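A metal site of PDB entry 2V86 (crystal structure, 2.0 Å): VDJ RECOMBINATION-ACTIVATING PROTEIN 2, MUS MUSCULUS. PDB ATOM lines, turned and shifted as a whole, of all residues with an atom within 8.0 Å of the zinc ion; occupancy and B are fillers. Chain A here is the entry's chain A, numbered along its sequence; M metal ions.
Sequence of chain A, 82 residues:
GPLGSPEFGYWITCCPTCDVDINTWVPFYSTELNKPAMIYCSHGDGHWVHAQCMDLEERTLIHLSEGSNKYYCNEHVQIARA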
ATOM      1  N   CYS A  14      16.241  -0.886 -22.386  1.00  0.00           N
ATOM      2  CA  CYS A  14      16.894  -2.200 -22.438  1.00  0.00           C
ATOM      3  C   CYS A  14      18.040  -2.383 -23.426  1.00  0.00           C
ATOM      4  O   CYS A  14      18.865  -3.262 -23.244  1.00  0.00           O
ATOM      5  CB  CYS A  14      15.845  -3.287 -22.684  1.00  0.00           C
ATOM      6  SG  CYS A  14      15.299  -3.435 -24.392  1.00  0.00           S
ATOM      7  N   CYS A  15      18.084  -1.568 -24.464  1.00  0.00           N
ATOM      8  CA  CYS A  15      19.149  -1.671 -25.464  1.00  0.00           C
ATOM      9  C   CYS A  15      19.187  -0.382 -26.280  1.00  0.00           C
ATOM     10  O   CYS A  15      18.270   0.407 -26.221  1.00  0.00           O
ATOM     11  CB  CYS A  15      18.895  -2.865 -26.383  1.00  0.00           C
ATOM     12  SG  CYS A  15      17.446  -2.698 -27.412  1.00  0.00           S
ATOM     13  N   ILE A  39      12.621 -10.674 -21.358  1.00  0.00           N
ATOM     14  CA  ILE A  39      13.385 -11.912 -21.406  1.00  0.00           C
ATOM     15  C   ILE A  39      14.711 -11.695 -20.697  1.00  0.00           C
ATOM     16  O   ILE A  39      15.313 -10.641 -20.823  1.00  0.00           O
ATOM     17  CB  ILE A  39      13.669 -12.328 -22.864  1.00  0.00           C
ATOM     18  CG1 ILE A  39      12.343 -12.561 -23.605  1.00  0.00           C
ATOM     19  CG2 ILE A  39      14.509 -13.590 -22.879  1.00  0.00           C
ATOM     20  CD1 ILE A  39      12.520 -12.785 -25.090  1.00  0.00           C
ATOM     21  N   TYR A  40      15.166 -12.704 -19.968  1.00  0.00           N
ATOM     22  CA  TYR A  40      16.427 -12.604 -19.247  1.00  0.00           C
ATOM     23  C   TYR A  40      17.574 -13.054 -20.155  1.00  0.00           C
ATOM     24  O   TYR A  40      17.567 -14.151 -20.684  1.00  0.00           O
ATOM     25  CB  TYR A  40      16.385 -13.473 -17.996  1.00  0.00           C
ATOM     26  CG  TYR A  40      17.652 -13.430 -17.158  1.00  0.00           C
ATOM     27  CD1 TYR A  40      18.042 -12.262 -16.493  1.00  0.00           C
ATOM     28  CD2 TYR A  40      18.447 -14.564 -17.000  1.00  0.00           C
ATOM     29  CE1 TYR A  40      19.186 -12.226 -15.699  1.00  0.00           C
ATOM     30  CE2 TYR A  40      19.592 -14.546 -16.217  1.00  0.00           C
ATOM     31  CZ  TYR A  40      19.960 -13.370 -15.568  1.00  0.00           C
ATOM     32  OH  TYR A  40      21.095 -13.353 -14.783  1.00  0.00           O
ATOM     33  N   CYS A  41      18.561 -12.184 -20.325  1.00  0.00           N
ATOM     34  CA  CYS A  41      19.735 -12.487 -21.141  1.00  0.00           C
ATOM     35  C   CYS A  41      20.843 -12.970 -20.219  1.00  0.00           C
ATOM     36  O   CYS A  41      21.161 -12.314 -19.244  1.00  0.00           O
ATOM     37  CB  CYS A  41      20.197 -11.236 -21.888  1.00  0.00           C
ATOM     38  SG  CYS A  41      21.803 -11.431 -22.705  1.00  0.00           S
ATOM     39  N   SER A  42      21.442 -14.102 -20.554  1.00  0.00           N
ATOM     40  CA  SER A  42      22.497 -14.703 -19.737  1.00  0.00           C
ATOM     41  C   SER A  42      23.908 -14.144 -19.925  1.00  0.00           C
ATOM     42  O   SER A  42      24.857 -14.732 -19.445  1.00  0.00           O
ATOM     43  CB  SER A  42      22.517 -16.222 -19.954  1.00  0.00           C
ATOM     44  OG  SER A  42      21.300 -16.804 -19.517  1.00  0.00           O
ATOM     45  N   HIS A  43      24.037 -13.023 -20.617  1.00  0.00           N
ATOM     46  CA  HIS A  43      25.357 -12.411 -20.831  1.00  0.00           C
ATOM     47  C   HIS A  43      25.913 -11.919 -19.496  1.00  0.00           C
ATOM     48  O   HIS A  43      25.251 -11.183 -18.787  1.00  0.00           O
ATOM     49  CB  HIS A  43      25.228 -11.230 -21.788  1.00  0.00           C
ATOM     50  CG  HIS A  43      26.523 -10.548 -22.086  1.00  0.00           C
ATOM     51  ND1 HIS A  43      27.513 -11.116 -22.852  1.00  0.00           N
ATOM     52  CD2 HIS A  43      26.988  -9.329 -21.716  1.00  0.00           C
ATOM     53  CE1 HIS A  43      28.529 -10.274 -22.950  1.00  0.00           C
ATOM     54  NE2 HIS A  43      28.232  -9.175 -22.271  1.00  0.00           N
ATOM     55  N   GLY A  44      27.134 -12.333 -19.154  1.00  0.00           N
ATOM     56  CA  GLY A  44      27.733 -11.907 -17.898  1.00  0.00           C
ATOM     57  C   GLY A  44      26.836 -12.220 -16.718  1.00  0.00           C
ATOM     58  O   GLY A  44      26.328 -13.319 -16.619  1.00  0.00           O
ATOM     59  N   GLY A  46      24.063 -11.205 -16.333  1.00  0.00           N
ATOM     60  CA  GLY A  46      22.687 -11.149 -16.821  1.00  0.00           C
ATOM     61  C   GLY A  46      21.945  -9.821 -16.725  1.00  0.00           C
ATOM     62  O   GLY A  46      22.230  -8.992 -15.891  1.00  0.00           O
ATOM     63  N   HIS A  47      20.970  -9.652 -17.625  1.00  0.00           N
ATOM     64  CA  HIS A  47      20.155  -8.448 -17.647  1.00  0.00           C
ATOM     65  C   HIS A  47      18.851  -8.761 -18.366  1.00  0.00           C
ATOM     66  O   HIS A  47      18.733  -9.769 -19.025  1.00  0.00           O
ATOM     67  CB  HIS A  47      20.886  -7.288 -18.334  1.00  0.00           C
ATOM     68  CG  HIS A  47      21.088  -7.460 -19.805  1.00  0.00           C
ATOM     69  ND1 HIS A  47      20.555  -6.593 -20.742  1.00  0.00           N
ATOM     70  CD2 HIS A  47      21.783  -8.377 -20.518  1.00  0.00           C
ATOM     71  CE1 HIS A  47      20.922  -6.968 -21.958  1.00  0.00           C
ATOM     72  NE2 HIS A  47      21.668  -8.055 -21.848  1.00  0.00           N
ATOM     73  N   TRP A  48      17.857  -7.878 -18.221  1.00  0.00           N
ATOM     74  CA  TRP A  48      16.567  -8.100 -18.856  1.00  0.00           C
ATOM     75  C   TRP A  48      16.354  -7.189 -20.058  1.00  0.00           C
ATOM     76  O   TRP A  48      16.752  -6.039 -20.042  1.00  0.00           O
ATOM     77  CB  TRP A  48      15.434  -7.849 -17.843  1.00  0.00           C
ATOM     78  CG  TRP A  48      15.378  -8.834 -16.713  1.00  0.00           C
ATOM     79  CD1 TRP A  48      16.103  -8.810 -15.565  1.00  0.00           C
ATOM     80  CD2 TRP A  48      14.545 -10.004 -16.643  1.00  0.00           C
ATOM     81  NE1 TRP A  48      15.774  -9.889 -14.774  1.00  0.00           N
ATOM     82  CE2 TRP A  48      14.825 -10.641 -15.423  1.00  0.00           C
ATOM     83  CE3 TRP A  48      13.598 -10.575 -17.503  1.00  0.00           C
ATOM     84  CZ2 TRP A  48      14.187 -11.820 -15.026  1.00  0.00           C
ATOM     85  CZ3 TRP A  48      12.959 -11.749 -17.115  1.00  0.00           C
ATOM     86  CH2 TRP A  48      13.256 -12.358 -15.881  1.00  0.00           C
ATOM     87  N   VAL A  49      15.745  -7.738 -21.104  1.00  0.00           N
ATOM     88  CA  VAL A  49      15.456  -6.941 -22.302  1.00  0.00           C
ATOM     89  C   VAL A  49      13.985  -7.094 -22.663  1.00  0.00           C
ATOM     90  O   VAL A  49      13.367  -8.073 -22.330  1.00  0.00           O
ATOM     91  CB  VAL A  49      16.316  -7.376 -23.519  1.00  0.00           C
ATOM     92  CG1 VAL A  49      17.772  -7.018 -23.294  1.00  0.00           C
ATOM     93  CG2 VAL A  49      16.161  -8.875 -23.756  1.00  0.00           C
ATOM     94  N   MET A  54      13.569  -6.909 -29.080  1.00  0.00           N
ATOM     95  CA  MET A  54      14.427  -7.925 -29.676  1.00  0.00           C
ATOM     96  C   MET A  54      13.845  -8.380 -31.021  1.00  0.00           C
ATOM     97  O   MET A  54      14.386  -9.246 -31.683  1.00  0.00           O
ATOM     98  CB  MET A  54      14.578  -9.121 -28.731  1.00  0.00           C
ATOM     99  CG  MET A  54      15.238  -8.805 -27.396  1.00  0.00           C
ATOM    100  SD  MET A  54      16.945  -8.176 -27.540  1.00  0.00           S
ATOM    101  CE  MET A  54      16.681  -6.396 -27.291  1.00  0.00           C
ATOM    102  N   TYR A  71      19.025 -17.653 -22.799  1.00  0.00           N
ATOM    103  CA  TYR A  71      18.788 -16.733 -23.901  1.00  0.00           C
ATOM    104  C   TYR A  71      19.836 -15.626 -23.910  1.00  0.00           C
ATOM    105  O   TYR A  71      20.238 -15.116 -22.868  1.00  0.00           O
ATOM    106  CB  TYR A  71      17.391 -16.112 -23.787  1.00  0.00           C
ATOM    107  CG  TYR A  71      17.152 -14.957 -24.754  1.00  0.00           C
ATOM    108  CD1 TYR A  71      17.324 -13.638 -24.343  1.00  0.00           C
ATOM    109  CD2 TYR A  71      16.757 -15.200 -26.075  1.00  0.00           C
ATOM    110  CE1 TYR A  71      17.112 -12.566 -25.223  1.00  0.00           C
ATOM    111  CE2 TYR A  71      16.555 -14.131 -26.969  1.00  0.00           C
ATOM    112  CZ  TYR A  71      16.730 -12.826 -26.532  1.00  0.00           C
ATOM    113  OH  TYR A  71      16.512 -11.775 -27.399  1.00  0.00           O
ATOM    114  N   TYR A  72      20.290 -15.259 -25.112  1.00  0.00           N
ATOM    115  CA  TYR A  72      21.251 -14.181 -25.264  1.00  0.00           C
ATOM    116  C   TYR A  72      20.617 -13.150 -26.199  1.00  0.00           C
ATOM    117  O   TYR A  72      20.208 -13.476 -27.298  1.00  0.00           O
ATOM    118  CB  TYR A  72      22.573 -14.707 -25.834  1.00  0.00           C
ATOM    119  CG  TYR A  72      23.314 -15.600 -24.860  1.00  0.00           C
ATOM    120  CD1 TYR A  72      23.138 -16.985 -24.879  1.00  0.00           C
ATOM    121  CD2 TYR A  72      24.160 -15.053 -23.896  1.00  0.00           C
ATOM    122  CE1 TYR A  72      23.785 -17.801 -23.952  1.00  0.00           C
ATOM    123  CE2 TYR A  72      24.816 -15.868 -22.970  1.00  0.00           C
ATOM    124  CZ  TYR A  72      24.616 -17.232 -23.008  1.00  0.00           C
ATOM    125  OH  TYR A  72      25.262 -18.044 -22.090  1.00  0.00           O
ATOM    126  N   CYS A  73      20.520 -11.914 -25.726  1.00  0.00           N
ATOM    127  CA  CYS A  73      19.903 -10.854 -26.508  1.00  0.00           C
ATOM    128  C   CYS A  73      20.703 -10.540 -27.766  1.00  0.00           C
ATOM    129  O   CYS A  73      21.854 -10.903 -27.883  1.00  0.00           O
ATOM    130  CB  CYS A  73      19.739  -9.591 -25.652  1.00  0.00           C
ATOM    131  SG  CYS A  73      21.263  -8.662 -25.402  1.00  0.00           S
ATOM    132  N   ASN A  74      20.063  -9.849 -28.695  1.00  0.00           N
ATOM    133  CA  ASN A  74      20.687  -9.506 -29.970  1.00  0.00           C
ATOM    134  C   ASN A  74      22.055  -8.850 -29.852  1.00  0.00           C
ATOM    135  O   ASN A  74      22.889  -8.979 -30.741  1.00  0.00           O
ATOM    136  CB  ASN A  74      19.726  -8.611 -30.760  1.00  0.00           C
ATOM    137  CG  ASN A  74      18.429  -9.330 -31.120  1.00  0.00           C
ATOM    138  OD1 ASN A  74      17.411  -8.714 -31.377  1.00  0.00           O
ATOM    139  ND2 ASN A  74      18.488 -10.653 -31.149  1.00  0.00           N
ATOM    140  N   GLU A  75      22.299  -8.175 -28.740  1.00  0.00           N
ATOM    141  CA  GLU A  75      23.583  -7.505 -28.499  1.00  0.00           C
ATOM    142  C   GLU A  75      24.679  -8.441 -28.017  1.00  0.00           C
ATOM    143  O   GLU A  75      25.853  -8.144 -28.169  1.00  0.00           O
ATOM    144  CB  GLU A  75      23.427  -6.422 -27.433  1.00  0.00           C
ATOM    145  CG  GLU A  75      23.161  -5.037 -27.941  1.00  0.00           C
ATOM    146  CD  GLU A  75      22.986  -4.074 -26.790  1.00  0.00           C
ATOM    147  OE1 GLU A  75      21.998  -4.231 -26.030  1.00  0.00           O
ATOM    148  OE2 GLU A  75      23.841  -3.178 -26.625  1.00  0.00           O
ATOM    149  N   HIS A  76      24.300  -9.568 -27.432  1.00  0.00           N
ATOM    150  CA  HIS A  76      25.287 -10.477 -26.873  1.00  0.00           C
ATOM    151  C   HIS A  76      25.323 -11.902 -27.409  1.00  0.00           C
ATOM    152  O   HIS A  76      26.266 -12.636 -27.139  1.00  0.00           O
ATOM    153  CB  HIS A  76      25.097 -10.527 -25.356  1.00  0.00           C
ATOM    154  CG  HIS A  76      25.139  -9.180 -24.714  1.00  0.00           C
ATOM    155  ND1 HIS A  76      24.224  -8.781 -23.764  1.00  0.00           N
ATOM    156  CD2 HIS A  76      25.993  -8.137 -24.882  1.00  0.00           C
ATOM    157  CE1 HIS A  76      24.518  -7.550 -23.363  1.00  0.00           C
ATOM    158  NE2 HIS A  76      25.580  -7.140 -24.026  1.00  0.00           N
ATOM    159  N   VAL A  77      24.300 -12.300 -28.159  1.00  0.00           N
ATOM    160  CA  VAL A  77      24.238 -13.662 -28.680  1.00  0.00           C
ATOM    161  C   VAL A  77      25.413 -14.018 -29.584  1.00  0.00           C
ATOM    162  O   VAL A  77      25.831 -15.159 -29.632  1.00  0.00           O
ATOM    163  CB  VAL A  77      22.914 -13.912 -29.430  1.00  0.00           C
ATOM    164  CG1 VAL A  77      22.789 -12.977 -30.620  1.00  0.00           C
ATOM    165  CG2 VAL A  77      22.830 -15.372 -29.864  1.00  0.00           C
HETATM  166 ZN    ZN M   1      22.205  -9.373 -23.392  1.00  0.00          ZN
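NE2 of His 47 binds the zinc ion. ND1 of His 76 binds the zinc ion (2.1 Å). SG of Cys 41 binds the zinc ion (2.2 Å). The side-chain sulfur (SG) of Cys 73 binds the zinc ion, at 2.3 Å. The zinc ion has four donor atoms within binding distance.
The side-chain sulfur (SG) of Cys 73 sits close to the backbone NH (N) of Glu 75, 3.5 Å away. The backbone NH of His 43 sits close to the side-chain sulfur of Cys 41, at 3.4 Å.
His 43 touches the zinc ion (CB to ZN, 3.9 Å). Within 4 Å of the zinc ion: Cys 41, His 43, His 47, Cys 73 and His 76. The nearest printed residue that does not touch the zinc ion is Tyr 72 (5.0 Å).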
